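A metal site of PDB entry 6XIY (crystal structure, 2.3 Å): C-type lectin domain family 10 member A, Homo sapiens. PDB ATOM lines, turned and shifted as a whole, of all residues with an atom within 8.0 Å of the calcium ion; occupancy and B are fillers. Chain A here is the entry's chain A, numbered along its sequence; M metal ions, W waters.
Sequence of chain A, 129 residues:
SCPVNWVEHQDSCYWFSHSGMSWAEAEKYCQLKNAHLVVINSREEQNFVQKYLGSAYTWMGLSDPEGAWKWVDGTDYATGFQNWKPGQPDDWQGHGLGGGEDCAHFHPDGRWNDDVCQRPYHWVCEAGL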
ATOM      1  N   HIS A   9      25.164  -2.935 -16.024  1.00  0.00           N
ATOM      2  CA  HIS A   9      25.333  -1.548 -16.538  1.00  0.00           C
ATOM      3  C   HIS A   9      26.845  -1.212 -16.543  1.00  0.00           C
ATOM      4  O   HIS A   9      27.453  -1.331 -15.467  1.00  0.00           O
ATOM      5  CB  HIS A   9      24.510  -0.555 -15.704  1.00  0.00           C
ATOM      6  CG  HIS A   9      24.847   0.886 -15.926  1.00  0.00           C
ATOM      7  ND1 HIS A   9      24.197   1.653 -16.886  1.00  0.00           N
ATOM      8  CD2 HIS A   9      25.734   1.709 -15.313  1.00  0.00           C
ATOM      9  CE1 HIS A   9      24.685   2.876 -16.861  1.00  0.00           C
ATOM     10  NE2 HIS A   9      25.625   2.932 -15.900  1.00  0.00           N
ATOM     11  N   GLN A  10      27.388  -0.867 -17.727  1.00  0.00           N
ATOM     12  CA  GLN A  10      28.736  -0.266 -17.993  1.00  0.00           C
ATOM     13  C   GLN A  10      29.834  -0.993 -17.190  1.00  0.00           C
ATOM     14  O   GLN A  10      30.546  -0.316 -16.401  1.00  0.00           O
ATOM     15  CB  GLN A  10      28.802   1.231 -17.676  1.00  0.00           C
ATOM     16  CG  GLN A  10      27.644   2.077 -18.218  1.00  0.00           C
ATOM     17  CD  GLN A  10      27.717   2.465 -19.673  1.00  0.00           C
ATOM     18  OE1 GLN A  10      28.525   1.961 -20.456  1.00  0.00           O
ATOM     19  NE2 GLN A  10      26.826   3.377 -20.070  1.00  0.00           N
ATOM     20  N   ASP A  11      29.975  -2.311 -17.383  1.00  0.00           N
ATOM     21  CA  ASP A  11      31.044  -3.166 -16.804  1.00  0.00           C
ATOM     22  C   ASP A  11      30.883  -3.315 -15.280  1.00  0.00           C
ATOM     23  O   ASP A  11      31.858  -3.727 -14.632  1.00  0.00           O
ATOM     24  CB  ASP A  11      32.435  -2.676 -17.226  1.00  0.00           C
ATOM     25  CG  ASP A  11      32.978  -3.479 -18.402  1.00  0.00           C
ATOM     26  OD1 ASP A  11      32.596  -3.168 -19.551  1.00  0.00           O
ATOM     27  OD2 ASP A  11      33.747  -4.446 -18.155  1.00  0.00           O
ATOM     28  N   SER A  12      29.695  -3.096 -14.723  1.00  0.00           N
ATOM     29  CA  SER A  12      29.382  -3.628 -13.368  1.00  0.00           C
ATOM     30  C   SER A  12      28.074  -4.411 -13.402  1.00  0.00           C
ATOM     31  O   SER A  12      27.259  -4.221 -14.339  1.00  0.00           O
ATOM     32  CB  SER A  12      29.326  -2.533 -12.361  1.00  0.00           C
ATOM     33  OG  SER A  12      30.618  -2.159 -11.960  1.00  0.00           O
ATOM     34  N   TYR A  14      24.826  -5.120 -10.676  1.00  0.00           N
ATOM     35  CA  TYR A  14      24.167  -4.536  -9.494  1.00  0.00           C
ATOM     36  C   TYR A  14      23.042  -5.450  -9.039  1.00  0.00           C
ATOM     37  O   TYR A  14      22.361  -6.022  -9.889  1.00  0.00           O
ATOM     38  CB  TYR A  14      23.656  -3.138  -9.824  1.00  0.00           C
ATOM     39  CG  TYR A  14      24.718  -2.190 -10.322  1.00  0.00           C
ATOM     40  CD1 TYR A  14      25.081  -2.182 -11.651  1.00  0.00           C
ATOM     41  CD2 TYR A  14      25.335  -1.311  -9.459  1.00  0.00           C
ATOM     42  CE1 TYR A  14      26.041  -1.308 -12.122  1.00  0.00           C
ATOM     43  CE2 TYR A  14      26.281  -0.405  -9.917  1.00  0.00           C
ATOM     44  CZ  TYR A  14      26.641  -0.420 -11.255  1.00  0.00           C
ATOM     45  OH  TYR A  14      27.583   0.440 -11.718  1.00  0.00           O
ATOM     46  N   HIS A  36      30.595  -5.793  -3.268  1.00  0.00           N
ATOM     47  CA  HIS A  36      30.805  -4.712  -2.281  1.00  0.00           C
ATOM     48  C   HIS A  36      29.569  -3.824  -2.314  1.00  0.00           C
ATOM     49  O   HIS A  36      28.874  -3.803  -3.340  1.00  0.00           O
ATOM     50  CB  HIS A  36      32.151  -4.013  -2.581  1.00  0.00           C
ATOM     51  CG  HIS A  36      32.236  -3.367  -3.933  1.00  0.00           C
ATOM     52  ND1 HIS A  36      31.580  -2.164  -4.242  1.00  0.00           N
ATOM     53  CD2 HIS A  36      32.886  -3.754  -5.065  1.00  0.00           C
ATOM     54  CE1 HIS A  36      31.827  -1.838  -5.505  1.00  0.00           C
ATOM     55  NE2 HIS A  36      32.626  -2.795  -6.035  1.00  0.00           N
ATOM     56  N   LEU A  37      29.284  -3.104  -1.229  1.00  0.00           N
ATOM     57  CA  LEU A  37      28.292  -2.010  -1.286  1.00  0.00           C
ATOM     58  C   LEU A  37      28.686  -1.104  -2.460  1.00  0.00           C
ATOM     59  O   LEU A  37      29.893  -0.860  -2.663  1.00  0.00           O
ATOM     60  CB  LEU A  37      28.239  -1.237   0.021  1.00  0.00           C
ATOM     61  CG  LEU A  37      27.509  -1.922   1.184  1.00  0.00           C
ATOM     62  CD1 LEU A  37      27.771  -1.150   2.456  1.00  0.00           C
ATOM     63  CD2 LEU A  37      26.017  -2.020   0.927  1.00  0.00           C
ATOM     64  N   VAL A  38      27.694  -0.619  -3.198  1.00  0.00           N
ATOM     65  CA  VAL A  38      27.902   0.186  -4.441  1.00  0.00           C
ATOM     66  C   VAL A  38      28.827   1.382  -4.123  1.00  0.00           C
ATOM     67  O   VAL A  38      28.637   2.084  -3.130  1.00  0.00           O
ATOM     68  CB  VAL A  38      26.537   0.582  -5.034  1.00  0.00           C
ATOM     69  CG1 VAL A  38      25.764   1.517  -4.099  1.00  0.00           C
ATOM     70  CG2 VAL A  38      26.671   1.186  -6.428  1.00  0.00           C
ATOM     71  N   VAL A  39      29.848   1.558  -4.957  1.00  0.00           N
ATOM     72  CA  VAL A  39      30.728   2.755  -5.027  1.00  0.00           C
ATOM     73  C   VAL A  39      30.249   3.584  -6.237  1.00  0.00           C
ATOM     74  O   VAL A  39      30.163   3.005  -7.348  1.00  0.00           O
ATOM     75  CB  VAL A  39      32.188   2.301  -5.173  1.00  0.00           C
ATOM     76  CG1 VAL A  39      33.136   3.446  -5.478  1.00  0.00           C
ATOM     77  CG2 VAL A  39      32.657   1.519  -3.965  1.00  0.00           C
ATOM     78  N   ILE A  40      29.984   4.865  -6.047  1.00  0.00           N
ATOM     79  CA  ILE A  40      29.491   5.764  -7.131  1.00  0.00           C
ATOM     80  C   ILE A  40      30.688   6.551  -7.676  1.00  0.00           C
ATOM     81  O   ILE A  40      31.201   7.439  -6.981  1.00  0.00           O
ATOM     82  CB  ILE A  40      28.328   6.644  -6.643  1.00  0.00           C
ATOM     83  CG1 ILE A  40      27.202   5.795  -6.052  1.00  0.00           C
ATOM     84  CG2 ILE A  40      27.819   7.513  -7.778  1.00  0.00           C
ATOM     85  CD1 ILE A  40      26.320   5.130  -7.098  1.00  0.00           C
ATOM     86  N   ASN A  41      31.105   6.202  -8.899  1.00  0.00           N
ATOM     87  CA  ASN A  41      32.366   6.674  -9.538  1.00  0.00           C
ATOM     88  C   ASN A  41      32.069   7.877 -10.433  1.00  0.00           C
ATOM     89  O   ASN A  41      32.999   8.630 -10.658  1.00  0.00           O
ATOM     90  CB  ASN A  41      33.076   5.548 -10.307  1.00  0.00           C
ATOM     91  CG  ASN A  41      33.455   4.372  -9.417  1.00  0.00           C
ATOM     92  OD1 ASN A  41      34.547   4.356  -8.831  1.00  0.00           O
ATOM     93  ND2 ASN A  41      32.549   3.421  -9.281  1.00  0.00           N
ATOM     94  N   SER A  42      30.816   8.084 -10.862  1.00  0.00           N
ATOM     95  CA  SER A  42      30.450   9.028 -11.951  1.00  0.00           C
ATOM     96  C   SER A  42      28.980   9.440 -11.851  1.00  0.00           C
ATOM     97  O   SER A  42      28.175   8.691 -11.251  1.00  0.00           O
ATOM     98  CB  SER A  42      30.729   8.423 -13.326  1.00  0.00           C
ATOM     99  OG  SER A  42      29.758   7.428 -13.659  1.00  0.00           O
ATOM    100  N   GLU A  45      26.759   6.725 -13.426  1.00  0.00           N
ATOM    101  CA  GLU A  45      26.470   5.603 -12.496  1.00  0.00           C
ATOM    102  C   GLU A  45      25.437   6.115 -11.454  1.00  0.00           C
ATOM    103  O   GLU A  45      24.481   5.384 -11.143  1.00  0.00           O
ATOM    104  CB  GLU A  45      27.777   5.030 -11.939  1.00  0.00           C
ATOM    105  CG  GLU A  45      27.578   3.867 -10.979  1.00  0.00           C
ATOM    106  CD  GLU A  45      28.819   3.145 -10.461  1.00  0.00           C
ATOM    107  OE1 GLU A  45      29.865   3.787 -10.242  1.00  0.00           O
ATOM    108  OE2 GLU A  45      28.748   1.915 -10.281  1.00  0.00           O
ATOM    109  N   GLN A  46      25.557   7.366 -10.991  1.00  0.00           N
ATOM    110  CA  GLN A  46      24.593   7.954 -10.027  1.00  0.00           C
ATOM    111  C   GLN A  46      23.192   7.952 -10.652  1.00  0.00           C
ATOM    112  O   GLN A  46      22.244   7.488  -9.983  1.00  0.00           O
ATOM    113  CB  GLN A  46      25.040   9.358  -9.600  1.00  0.00           C
ATOM    114  CG  GLN A  46      23.972  10.163  -8.884  1.00  0.00           C
ATOM    115  CD  GLN A  46      23.724   9.684  -7.471  1.00  0.00           C
ATOM    116  OE1 GLN A  46      24.639   9.248  -6.779  1.00  0.00           O
ATOM    117  NE2 GLN A  46      22.468   9.763  -7.032  1.00  0.00           N
ATOM    118  N   VAL A  49      21.748   4.298 -10.881  1.00  0.00           N
ATOM    119  CA  VAL A  49      21.345   3.758  -9.547  1.00  0.00           C
ATOM    120  C   VAL A  49      20.101   4.512  -9.064  1.00  0.00           C
ATOM    121  O   VAL A  49      19.142   3.862  -8.657  1.00  0.00           O
ATOM    122  CB  VAL A  49      22.522   3.831  -8.556  1.00  0.00           C
ATOM    123  CG1 VAL A  49      22.107   3.474  -7.143  1.00  0.00           C
ATOM    124  CG2 VAL A  49      23.675   2.941  -9.014  1.00  0.00           C
ATOM    125  N   TRP A  71      35.437   5.060   0.560  1.00  0.00           N
ATOM    126  CA  TRP A  71      34.653   4.078  -0.240  1.00  0.00           C
ATOM    127  C   TRP A  71      35.158   2.683   0.107  1.00  0.00           C
ATOM    128  O   TRP A  71      36.349   2.541   0.323  1.00  0.00           O
ATOM    129  CB  TRP A  71      34.809   4.357  -1.735  1.00  0.00           C
ATOM    130  CG  TRP A  71      34.146   5.604  -2.220  1.00  0.00           C
ATOM    131  CD1 TRP A  71      34.749   6.766  -2.597  1.00  0.00           C
ATOM    132  CD2 TRP A  71      32.731   5.818  -2.417  1.00  0.00           C
ATOM    133  NE1 TRP A  71      33.818   7.675  -3.008  1.00  0.00           N
ATOM    134  CE2 TRP A  71      32.574   7.114  -2.931  1.00  0.00           C
ATOM    135  CE3 TRP A  71      31.601   5.011  -2.276  1.00  0.00           C
ATOM    136  CZ2 TRP A  71      31.326   7.639  -3.272  1.00  0.00           C
ATOM    137  CZ3 TRP A  71      30.369   5.536  -2.598  1.00  0.00           C
ATOM    138  CH2 TRP A  71      30.240   6.825  -3.082  1.00  0.00           C
ATOM    139  N   ASP A  73      35.923   0.068  -1.513  1.00  0.00           N
ATOM    140  CA  ASP A  73      36.903  -0.568  -2.449  1.00  0.00           C
ATOM    141  C   ASP A  73      38.177   0.281  -2.562  1.00  0.00           C
ATOM    142  O   ASP A  73      39.074  -0.135  -3.316  1.00  0.00           O
ATOM    143  CB  ASP A  73      36.251  -0.818  -3.807  1.00  0.00           C
ATOM    144  CG  ASP A  73      36.107   0.440  -4.673  1.00  0.00           C
ATOM    145  OD1 ASP A  73      36.258   1.554  -4.106  1.00  0.00           O
ATOM    146  OD2 ASP A  73      35.859   0.302  -5.899  1.00  0.00           O
ATOM    147  N   THR A  75      38.372   3.540  -3.783  1.00  0.00           N
ATOM    148  CA  THR A  75      38.186   4.741  -4.647  1.00  0.00           C
ATOM    149  C   THR A  75      38.433   5.995  -3.795  1.00  0.00           C
ATOM    150  O   THR A  75      37.938   6.034  -2.646  1.00  0.00           O
ATOM    151  CB  THR A  75      36.784   4.756  -5.271  1.00  0.00           C
ATOM    152  OG1 THR A  75      36.638   3.591  -6.090  1.00  0.00           O
ATOM    153  CG2 THR A  75      36.497   6.018  -6.061  1.00  0.00           C
ATOM    154  N   GLU A 126      27.479  -4.087  -5.808  1.00  0.00           N
ATOM    155  CA  GLU A 126      28.154  -3.893  -7.118  1.00  0.00           C
ATOM    156  C   GLU A 126      29.249  -4.962  -7.222  1.00  0.00           C
ATOM    157  O   GLU A 126      29.941  -5.174  -6.214  1.00  0.00           O
ATOM    158  CB  GLU A 126      28.723  -2.465  -7.166  1.00  0.00           C
ATOM    159  CG  GLU A 126      29.601  -2.156  -8.372  1.00  0.00           C
ATOM    160  CD  GLU A 126      30.035  -0.703  -8.654  1.00  0.00           C
ATOM    161  OE1 GLU A 126      30.112   0.153  -7.716  1.00  0.00           O
ATOM    162  OE2 GLU A 126      30.354  -0.407  -9.838  1.00  0.00           O
ATOM    163  N   ALA A 127      29.413  -5.618  -8.379  1.00  0.00           N
ATOM    164  CA  ALA A 127      30.589  -6.481  -8.701  1.00  0.00           C
ATOM    165  C   ALA A 127      31.017  -6.234 -10.149  1.00  0.00           C
ATOM    166  O   ALA A 127      30.217  -5.652 -10.934  1.00  0.00           O
ATOM    167  CB  ALA A 127      30.227  -7.932  -8.512  1.00  0.00           C
HETATM  168 CA    CA M   1      30.847   1.823  -9.280  1.00  0.00          CA
HETATM  169  O   HOH W   1      31.602   1.815 -11.463  1.00  0.00           O
HETATM  170  O   HOH W   2      32.628   0.522  -8.500  1.00  0.00           O
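The side-chain carboxylate (OE2) of Glu 126 lies close to the side-chain hydroxyl (OH) of Tyr 14. OE2 of Glu 126 sits close to OG of Ser 12 (2.8 Å). N of Glu 126 is in hydrogen-bond range of O of His 36 (2.8 Å). N of Glu 45 lies within hydrogen-bond range of OG of Ser 42, 3.1 Å away.
Of the 20 residues printed, 4 come within 4 Å of the calcium ion. The nearest printed residue that does not touch the calcium ion is Tyr 14 (4.3 Å).
The calcium ion is bound by water W1, the side-chain carboxylate (OE2) of Glu 45, the side-chain amide nitrogen (ND2) of Asn 41, water W2, the side-chain carboxylate (OE2) of Glu 126, the backbone carbonyl oxygen (O) of Val 39, the side-chain carboxylate (OE1) of Glu 45 and the side-chain carboxylate (OE1) of Glu 126.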
